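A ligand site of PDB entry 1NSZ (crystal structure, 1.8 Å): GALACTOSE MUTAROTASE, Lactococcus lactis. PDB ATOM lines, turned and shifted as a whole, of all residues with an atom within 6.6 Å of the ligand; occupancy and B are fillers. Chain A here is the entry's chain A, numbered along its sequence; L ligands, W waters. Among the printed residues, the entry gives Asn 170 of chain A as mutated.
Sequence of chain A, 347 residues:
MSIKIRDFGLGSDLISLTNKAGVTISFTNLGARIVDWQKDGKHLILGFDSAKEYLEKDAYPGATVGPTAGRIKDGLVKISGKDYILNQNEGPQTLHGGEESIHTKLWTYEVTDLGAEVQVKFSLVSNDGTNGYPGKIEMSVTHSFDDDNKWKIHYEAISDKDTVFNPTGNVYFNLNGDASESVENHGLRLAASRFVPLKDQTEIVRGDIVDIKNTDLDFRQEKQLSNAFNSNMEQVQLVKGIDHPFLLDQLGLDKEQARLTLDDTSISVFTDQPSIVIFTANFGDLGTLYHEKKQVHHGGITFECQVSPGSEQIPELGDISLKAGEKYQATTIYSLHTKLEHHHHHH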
ATOM      1  N   ASP A  58      29.914 -17.912 -30.612  1.00  0.00           N
ATOM      2  CA  ASP A  58      29.207 -18.262 -29.401  1.00  0.00           C
ATOM      3  C   ASP A  58      27.777 -18.470 -29.848  1.00  0.00           C
ATOM      4  O   ASP A  58      27.159 -17.542 -30.368  1.00  0.00           O
ATOM      5  CB  ASP A  58      29.345 -17.200 -28.306  1.00  0.00           C
ATOM      6  CG  ASP A  58      28.595 -17.592 -27.060  1.00  0.00           C
ATOM      7  OD1 ASP A  58      27.914 -18.593 -26.941  1.00  0.00           O
ATOM      8  OD2 ASP A  58      28.723 -16.734 -26.103  1.00  0.00           O
ATOM      9  N   TYR A  60      25.204 -19.328 -28.040  1.00  0.00           N
ATOM     10  CA  TYR A  60      24.158 -19.108 -27.034  1.00  0.00           C
ATOM     11  C   TYR A  60      23.410 -17.798 -27.059  1.00  0.00           C
ATOM     12  O   TYR A  60      22.195 -17.766 -26.761  1.00  0.00           O
ATOM     13  CB  TYR A  60      24.722 -19.308 -25.613  1.00  0.00           C
ATOM     14  CG  TYR A  60      24.972 -20.767 -25.280  1.00  0.00           C
ATOM     15  CD1 TYR A  60      26.146 -21.172 -24.627  1.00  0.00           C
ATOM     16  CD2 TYR A  60      24.033 -21.751 -25.600  1.00  0.00           C
ATOM     17  CE1 TYR A  60      26.407 -22.499 -24.307  1.00  0.00           C
ATOM     18  CE2 TYR A  60      24.272 -23.095 -25.293  1.00  0.00           C
ATOM     19  CZ  TYR A  60      25.449 -23.470 -24.636  1.00  0.00           C
ATOM     20  OH  TYR A  60      25.701 -24.774 -24.333  1.00  0.00           O
ATOM     21  N   PRO A  61      24.115 -16.708 -27.338  1.00  0.00           N
ATOM     22  CA  PRO A  61      23.469 -15.399 -27.263  1.00  0.00           C
ATOM     23  C   PRO A  61      22.134 -15.234 -27.996  1.00  0.00           C
ATOM     24  O   PRO A  61      22.092 -15.462 -29.185  1.00  0.00           O
ATOM     25  CB  PRO A  61      24.519 -14.364 -27.653  1.00  0.00           C
ATOM     26  CG  PRO A  61      25.866 -15.090 -27.598  1.00  0.00           C
ATOM     27  CD  PRO A  61      25.564 -16.570 -27.696  1.00  0.00           C
ATOM     28  N   GLY A  70      20.418 -24.464 -18.144  1.00  0.00           N
ATOM     29  CA  GLY A  70      21.270 -24.513 -16.978  1.00  0.00           C
ATOM     30  C   GLY A  70      22.072 -25.794 -16.900  1.00  0.00           C
ATOM     31  O   GLY A  70      22.078 -26.605 -17.832  1.00  0.00           O
ATOM     32  N   ARG A  71      22.774 -25.949 -15.756  1.00  0.00           N
ATOM     33  CA  ARG A  71      23.587 -27.121 -15.512  1.00  0.00           C
ATOM     34  C   ARG A  71      22.896 -28.179 -14.705  1.00  0.00           C
ATOM     35  O   ARG A  71      22.300 -27.862 -13.640  1.00  0.00           O
ATOM     36  CB  ARG A  71      24.787 -26.752 -14.669  1.00  0.00           C
ATOM     37  CG  ARG A  71      25.706 -25.878 -15.451  1.00  0.00           C
ATOM     38  CD  ARG A  71      26.924 -25.397 -14.634  1.00  0.00           C
ATOM     39  NE  ARG A  71      27.758 -24.652 -15.614  1.00  0.00           N
ATOM     40  CZ  ARG A  71      27.652 -23.380 -15.993  1.00  0.00           C
ATOM     41  NH1 ARG A  71      26.770 -22.508 -15.438  1.00  0.00           N
ATOM     42  NH2 ARG A  71      28.508 -22.996 -16.939  1.00  0.00           N
ATOM     43  N   GLU A  90      29.941 -30.362 -20.528  1.00  0.00           N
ATOM     44  CA  GLU A  90      30.773 -29.436 -19.770  1.00  0.00           C
ATOM     45  C   GLU A  90      31.299 -30.271 -18.653  1.00  0.00           C
ATOM     46  O   GLU A  90      30.705 -30.313 -17.554  1.00  0.00           O
ATOM     47  CB  GLU A  90      29.933 -28.284 -19.220  1.00  0.00           C
ATOM     48  CG  GLU A  90      30.864 -27.211 -18.646  1.00  0.00           C
ATOM     49  CD  GLU A  90      30.098 -26.212 -17.814  1.00  0.00           C
ATOM     50  OE1 GLU A  90      29.447 -26.554 -16.864  1.00  0.00           O
ATOM     51  OE2 GLU A  90      30.210 -24.978 -18.199  1.00  0.00           O
ATOM     52  N   LEU A  95      24.971 -28.983 -19.699  1.00  0.00           N
ATOM     53  CA  LEU A  95      24.695 -27.542 -19.711  1.00  0.00           C
ATOM     54  C   LEU A  95      23.796 -27.204 -20.890  1.00  0.00           C
ATOM     55  O   LEU A  95      24.121 -27.510 -22.021  1.00  0.00           O
ATOM     56  CB  LEU A  95      26.020 -26.748 -19.893  1.00  0.00           C
ATOM     57  CG  LEU A  95      25.826 -25.227 -20.188  1.00  0.00           C
ATOM     58  CD1 LEU A  95      25.156 -24.482 -19.027  1.00  0.00           C
ATOM     59  CD2 LEU A  95      27.159 -24.556 -20.446  1.00  0.00           C
ATOM     60  N   HIS A  96      22.689 -26.557 -20.644  1.00  0.00           N
ATOM     61  CA  HIS A  96      21.806 -26.166 -21.776  1.00  0.00           C
ATOM     62  C   HIS A  96      21.435 -27.283 -22.754  1.00  0.00           C
ATOM     63  O   HIS A  96      21.475 -27.106 -24.002  1.00  0.00           O
ATOM     64  CB  HIS A  96      22.408 -24.982 -22.556  1.00  0.00           C
ATOM     65  CG  HIS A  96      22.376 -23.694 -21.773  1.00  0.00           C
ATOM     66  ND1 HIS A  96      21.636 -23.585 -20.572  1.00  0.00           N
ATOM     67  CD2 HIS A  96      22.969 -22.507 -22.028  1.00  0.00           C
ATOM     68  CE1 HIS A  96      21.803 -22.359 -20.143  1.00  0.00           C
ATOM     69  NE2 HIS A  96      22.595 -21.669 -20.988  1.00  0.00           N
ATOM     70  N   THR A 168      14.742 -21.821 -21.723  1.00  0.00           N
ATOM     71  CA  THR A 168      14.823 -20.390 -21.417  1.00  0.00           C
ATOM     72  C   THR A 168      15.341 -19.641 -22.626  1.00  0.00           C
ATOM     73  O   THR A 168      15.783 -20.269 -23.609  1.00  0.00           O
ATOM     74  CB  THR A 168      15.580 -20.038 -20.088  1.00  0.00           C
ATOM     75  OG1 THR A 168      15.191 -18.746 -19.655  1.00  0.00           O
ATOM     76  CG2 THR A 168      17.109 -20.069 -20.287  1.00  0.00           C
ATOM     77  N   ASN A 170      18.059 -16.858 -23.914  1.00  0.00           N
ATOM     78  CA  ASN A 170      19.386 -16.420 -23.536  1.00  0.00           C
ATOM     79  C   ASN A 170      19.857 -15.055 -24.069  1.00  0.00           C
ATOM     80  O   ASN A 170      21.041 -14.859 -24.388  1.00  0.00           O
ATOM     81  CB  ASN A 170      20.383 -17.523 -23.940  1.00  0.00           C
ATOM     82  CG  ASN A 170      21.579 -17.722 -23.009  1.00  0.00           C
ATOM     83  OD1 ASN A 170      21.725 -18.790 -22.433  1.00  0.00           O
ATOM     84  ND2 ASN A 170      22.509 -16.785 -22.956  1.00  0.00           N
ATOM     85  N   TYR A 172      21.230 -11.342 -24.095  1.00  0.00           N
ATOM     86  CA  TYR A 172      22.143 -10.555 -23.255  1.00  0.00           C
ATOM     87  C   TYR A 172      21.844  -9.083 -23.566  1.00  0.00           C
ATOM     88  O   TYR A 172      21.856  -8.640 -24.739  1.00  0.00           O
ATOM     89  CB  TYR A 172      23.617 -10.716 -23.663  1.00  0.00           C
ATOM     90  CG  TYR A 172      24.315 -11.992 -23.239  1.00  0.00           C
ATOM     91  CD1 TYR A 172      24.267 -13.143 -24.013  1.00  0.00           C
ATOM     92  CD2 TYR A 172      25.078 -12.014 -22.069  1.00  0.00           C
ATOM     93  CE1 TYR A 172      24.974 -14.290 -23.654  1.00  0.00           C
ATOM     94  CE2 TYR A 172      25.787 -13.154 -21.689  1.00  0.00           C
ATOM     95  CZ  TYR A 172      25.739 -14.302 -22.483  1.00  0.00           C
ATOM     96  OH  TYR A 172      26.438 -15.431 -22.101  1.00  0.00           O
ATOM     97  N   GLU A 203      30.340 -24.745 -10.981  1.00  0.00           N
ATOM     98  CA  GLU A 203      29.077 -24.079 -11.094  1.00  0.00           C
ATOM     99  C   GLU A 203      27.851 -24.899 -10.847  1.00  0.00           C
ATOM    100  O   GLU A 203      26.764 -24.478 -11.216  1.00  0.00           O
ATOM    101  CB  GLU A 203      28.960 -23.229 -12.355  1.00  0.00           C
ATOM    102  CG  GLU A 203      29.987 -22.072 -12.345  1.00  0.00           C
ATOM    103  CD  GLU A 203      30.128 -21.252 -13.612  1.00  0.00           C
ATOM    104  OE1 GLU A 203      31.091 -21.324 -14.386  1.00  0.00           O
ATOM    105  OE2 GLU A 203      29.152 -20.383 -13.762  1.00  0.00           O
ATOM    106  N   ASP A 243      26.358 -14.998 -11.587  1.00  0.00           N
ATOM    107  CA  ASP A 243      26.056 -16.170 -12.422  1.00  0.00           C
ATOM    108  C   ASP A 243      25.188 -17.056 -11.581  1.00  0.00           C
ATOM    109  O   ASP A 243      25.599 -18.145 -11.252  1.00  0.00           O
ATOM    110  CB  ASP A 243      27.308 -16.964 -12.879  1.00  0.00           C
ATOM    111  CG  ASP A 243      26.983 -17.836 -14.068  1.00  0.00           C
ATOM    112  OD1 ASP A 243      25.871 -17.944 -14.556  1.00  0.00           O
ATOM    113  OD2 ASP A 243      28.010 -18.420 -14.597  1.00  0.00           O
ATOM    114  N   HIS A 244      24.013 -16.540 -11.221  1.00  0.00           N
ATOM    115  CA  HIS A 244      23.191 -17.249 -10.287  1.00  0.00           C
ATOM    116  C   HIS A 244      21.715 -17.092 -10.475  1.00  0.00           C
ATOM    117  O   HIS A 244      21.235 -16.076 -10.984  1.00  0.00           O
ATOM    118  CB  HIS A 244      23.366 -16.528  -8.934  1.00  0.00           C
ATOM    119  CG  HIS A 244      24.740 -16.676  -8.351  1.00  0.00           C
ATOM    120  ND1 HIS A 244      25.821 -15.875  -8.751  1.00  0.00           N
ATOM    121  CD2 HIS A 244      25.162 -17.532  -7.397  1.00  0.00           C
ATOM    122  CE1 HIS A 244      26.876 -16.274  -8.066  1.00  0.00           C
ATOM    123  NE2 HIS A 244      26.501 -17.260  -7.233  1.00  0.00           N
ATOM    124  N   VAL A 277      17.771 -16.413 -13.830  1.00  0.00           N
ATOM    125  CA  VAL A 277      19.179 -16.641 -13.751  1.00  0.00           C
ATOM    126  C   VAL A 277      19.897 -15.429 -14.357  1.00  0.00           C
ATOM    127  O   VAL A 277      19.664 -15.047 -15.525  1.00  0.00           O
ATOM    128  CB  VAL A 277      19.580 -17.973 -14.432  1.00  0.00           C
ATOM    129  CG1 VAL A 277      21.107 -18.085 -14.389  1.00  0.00           C
ATOM    130  CG2 VAL A 277      18.889 -19.133 -13.698  1.00  0.00           C
ATOM    131  N   ILE A 278      20.775 -14.816 -13.559  1.00  0.00           N
ATOM    132  CA  ILE A 278      21.474 -13.621 -14.016  1.00  0.00           C
ATOM    133  C   ILE A 278      22.915 -13.879 -14.204  1.00  0.00           C
ATOM    134  O   ILE A 278      23.594 -14.270 -13.252  1.00  0.00           O
ATOM    135  CB  ILE A 278      21.273 -12.512 -12.993  1.00  0.00           C
ATOM    136  CG1 ILE A 278      19.784 -12.188 -12.978  1.00  0.00           C
ATOM    137  CG2 ILE A 278      22.119 -11.267 -13.314  1.00  0.00           C
ATOM    138  CD1 ILE A 278      19.440 -11.078 -12.024  1.00  0.00           C
ATOM    139  N   PHE A 279      23.369 -13.668 -15.431  1.00  0.00           N
ATOM    140  CA  PHE A 279      24.780 -13.896 -15.746  1.00  0.00           C
ATOM    141  C   PHE A 279      25.340 -12.638 -16.374  1.00  0.00           C
ATOM    142  O   PHE A 279      24.770 -12.132 -17.342  1.00  0.00           O
ATOM    143  CB  PHE A 279      24.931 -15.161 -16.627  1.00  0.00           C
ATOM    144  CG  PHE A 279      26.287 -15.363 -17.271  1.00  0.00           C
ATOM    145  CD1 PHE A 279      27.407 -15.609 -16.476  1.00  0.00           C
ATOM    146  CD2 PHE A 279      26.404 -15.315 -18.657  1.00  0.00           C
ATOM    147  CE1 PHE A 279      28.652 -15.828 -17.070  1.00  0.00           C
ATOM    148  CE2 PHE A 279      27.642 -15.501 -19.267  1.00  0.00           C
ATOM    149  CZ  PHE A 279      28.750 -15.768 -18.465  1.00  0.00           C
ATOM    150  N   PHE A 283      33.444 -13.069 -18.884  1.00  0.00           N
ATOM    151  CA  PHE A 283      34.416 -13.743 -19.777  1.00  0.00           C
ATOM    152  C   PHE A 283      35.876 -13.327 -19.706  1.00  0.00           C
ATOM    153  O   PHE A 283      36.691 -13.721 -20.551  1.00  0.00           O
ATOM    154  CB  PHE A 283      33.984 -13.639 -21.252  1.00  0.00           C
ATOM    155  CG  PHE A 283      32.582 -14.182 -21.471  1.00  0.00           C
ATOM    156  CD1 PHE A 283      31.520 -13.332 -21.805  1.00  0.00           C
ATOM    157  CD2 PHE A 283      32.313 -15.550 -21.353  1.00  0.00           C
ATOM    158  CE1 PHE A 283      30.230 -13.843 -22.031  1.00  0.00           C
ATOM    159  CE2 PHE A 283      31.032 -16.075 -21.561  1.00  0.00           C
ATOM    160  CZ  PHE A 283      29.992 -15.207 -21.893  1.00  0.00           C
ATOM    161  N   THR A 302      22.251 -11.212 -18.612  1.00  0.00           N
ATOM    162  CA  THR A 302      21.075 -12.017 -18.988  1.00  0.00           C
ATOM    163  C   THR A 302      19.986 -11.959 -17.952  1.00  0.00           C
ATOM    164  O   THR A 302      20.261 -11.685 -16.800  1.00  0.00           O
ATOM    165  CB  THR A 302      21.442 -13.528 -19.116  1.00  0.00           C
ATOM    166  OG1 THR A 302      21.739 -14.024 -17.812  1.00  0.00           O
ATOM    167  CG2 THR A 302      22.616 -13.798 -20.059  1.00  0.00           C
ATOM    168  N   GLU A 304      17.548 -14.913 -17.556  1.00  0.00           N
ATOM    169  CA  GLU A 304      17.013 -16.207 -18.001  1.00  0.00           C
ATOM    170  C   GLU A 304      15.881 -16.655 -17.091  1.00  0.00           C
ATOM    171  O   GLU A 304      16.095 -17.129 -15.985  1.00  0.00           O
ATOM    172  CB  GLU A 304      18.166 -17.227 -17.972  1.00  0.00           C
ATOM    173  CG  GLU A 304      19.236 -16.883 -19.057  1.00  0.00           C
ATOM    174  CD  GLU A 304      20.564 -17.617 -18.932  1.00  0.00           C
ATOM    175  OE1 GLU A 304      20.777 -18.520 -18.184  1.00  0.00           O
ATOM    176  OE2 GLU A 304      21.455 -17.189 -19.762  1.00  0.00           O
ATOM    177  N   GLN A 306      13.152 -19.089 -15.758  1.00  0.00           N
ATOM    178  CA  GLN A 306      12.894 -20.537 -15.812  1.00  0.00           C
ATOM    179  C   GLN A 306      12.749 -21.065 -14.366  1.00  0.00           C
ATOM    180  O   GLN A 306      12.748 -20.319 -13.403  1.00  0.00           O
ATOM    181  CB  GLN A 306      14.162 -21.225 -16.397  1.00  0.00           C
ATOM    182  CG  GLN A 306      15.427 -20.786 -15.595  1.00  0.00           C
ATOM    183  CD  GLN A 306      16.695 -21.518 -15.994  1.00  0.00           C
ATOM    184  OE1 GLN A 306      17.505 -20.977 -16.788  1.00  0.00           O
ATOM    185  NE2 GLN A 306      16.874 -22.767 -15.522  1.00  0.00           N
HETATM  186  C1  LIG L   1      27.636 -19.409 -18.856  1.00  0.00           C
HETATM  187  C2  LIG L   1      26.938 -19.180 -17.509  1.00  0.00           C
HETATM  188  C3  LIG L   1      25.548 -19.737 -17.548  1.00  0.00           C
HETATM  189  C4  LIG L   1      24.790 -19.033 -18.680  1.00  0.00           C
HETATM  190  C5  LIG L   1      25.484 -19.439 -19.980  1.00  0.00           C
HETATM  191  C6  LIG L   1      24.942 -18.766 -21.239  1.00  0.00           C
HETATM  192  O1  LIG L   1      27.861 -20.805 -18.999  1.00  0.00           O
HETATM  193  O2  LIG L   1      27.634 -19.873 -16.506  1.00  0.00           O
HETATM  194  O3  LIG L   1      24.957 -19.531 -16.256  1.00  0.00           O
HETATM  195  O4  LIG L   1      23.409 -19.332 -18.767  1.00  0.00           O
HETATM  196  O5  LIG L   1      26.848 -18.959 -19.950  1.00  0.00           O
HETATM  197  O6  LIG L   1      24.408 -17.506 -20.859  1.00  0.00           O
HETATM  198  O   HOH W   1      22.680 -21.366 -15.857  1.00  0.00           O
HETATM  199  O   HOH W   2      30.203 -19.652 -16.894  1.00  0.00           O
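OD2 of Asp 243 sits at hydrogen-bond distance from O2 of the ligand, at 2.4 Å.
A ring nitrogen (NE2) of His 96 lies within hydrogen-bond range of an oxygen (O4) of the ligand, at 3.3 Å.
ND2 of Asn 170 lies within hydrogen-bond range of O6 of the ligand (2.9 Å).
OH of Tyr 172 lies within hydrogen-bond range of O6 of the ligand (3.2 Å).
NH1 of Arg 71 sits at hydrogen-bond distance from O2 of the ligand.
An oxygen (O2) of the ligand sits at hydrogen-bond distance from the side-chain carboxylate (OE2) of Glu 203, at 3.2 Å.
An oxygen (O4) of the ligand is in hydrogen-bond range of the side-chain carboxylate of Glu 304.
The backbone carbonyl oxygen (O) of Glu 304 lies within hydrogen-bond range of the backbone NH (N) of Val 277 (2.8 Å).
ND1 of His 96 sits at hydrogen-bond distance from N of Gly 70 (2.9 Å).
The side-chain carboxylate (OD2) of Asp 243 lies close to the side-chain carboxylate (OE2) of Glu 203, at 2.4 Å.
The side-chain amide oxygen (OD1) of Asn 170 sits at hydrogen-bond distance from a ring nitrogen (NE2) of His 96 (3.3 Å).
The guanidinium group (NH1) of Arg 71 is in salt-bridge range of the side-chain carboxylate (OE2) of Glu 203, 3.6 Å away.
The guanidinium group (NE) of Arg 71 is in salt-bridge range of the side-chain carboxylate (OE1) of Glu 90 (2.8 Å).
The backbone NH (N) of Phe 279 sits at hydrogen-bond distance from the side-chain hydroxyl (OG1) of Thr 302 (2.9 Å).
The backbone NH (N) of Asp 243 lies close to the backbone carbonyl oxygen (O) of Ile 278 (3.3 Å).
CE2 of Phe 279 touches O5 of the ligand (3.6 Å).
Hydrophobic or aromatic side chains that line the ligand: His 96, Tyr 172 and Phe 279.
Of the 21 residues printed, 8 come within 4 Å of the ligand.
Water W2 lies within hydrogen-bond range of an oxygen (O2) of the ligand (2.6 Å), the side-chain carboxylate of Glu 203 (3.1 Å) and the side-chain carboxylate of Asp 243 (3.4 Å).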
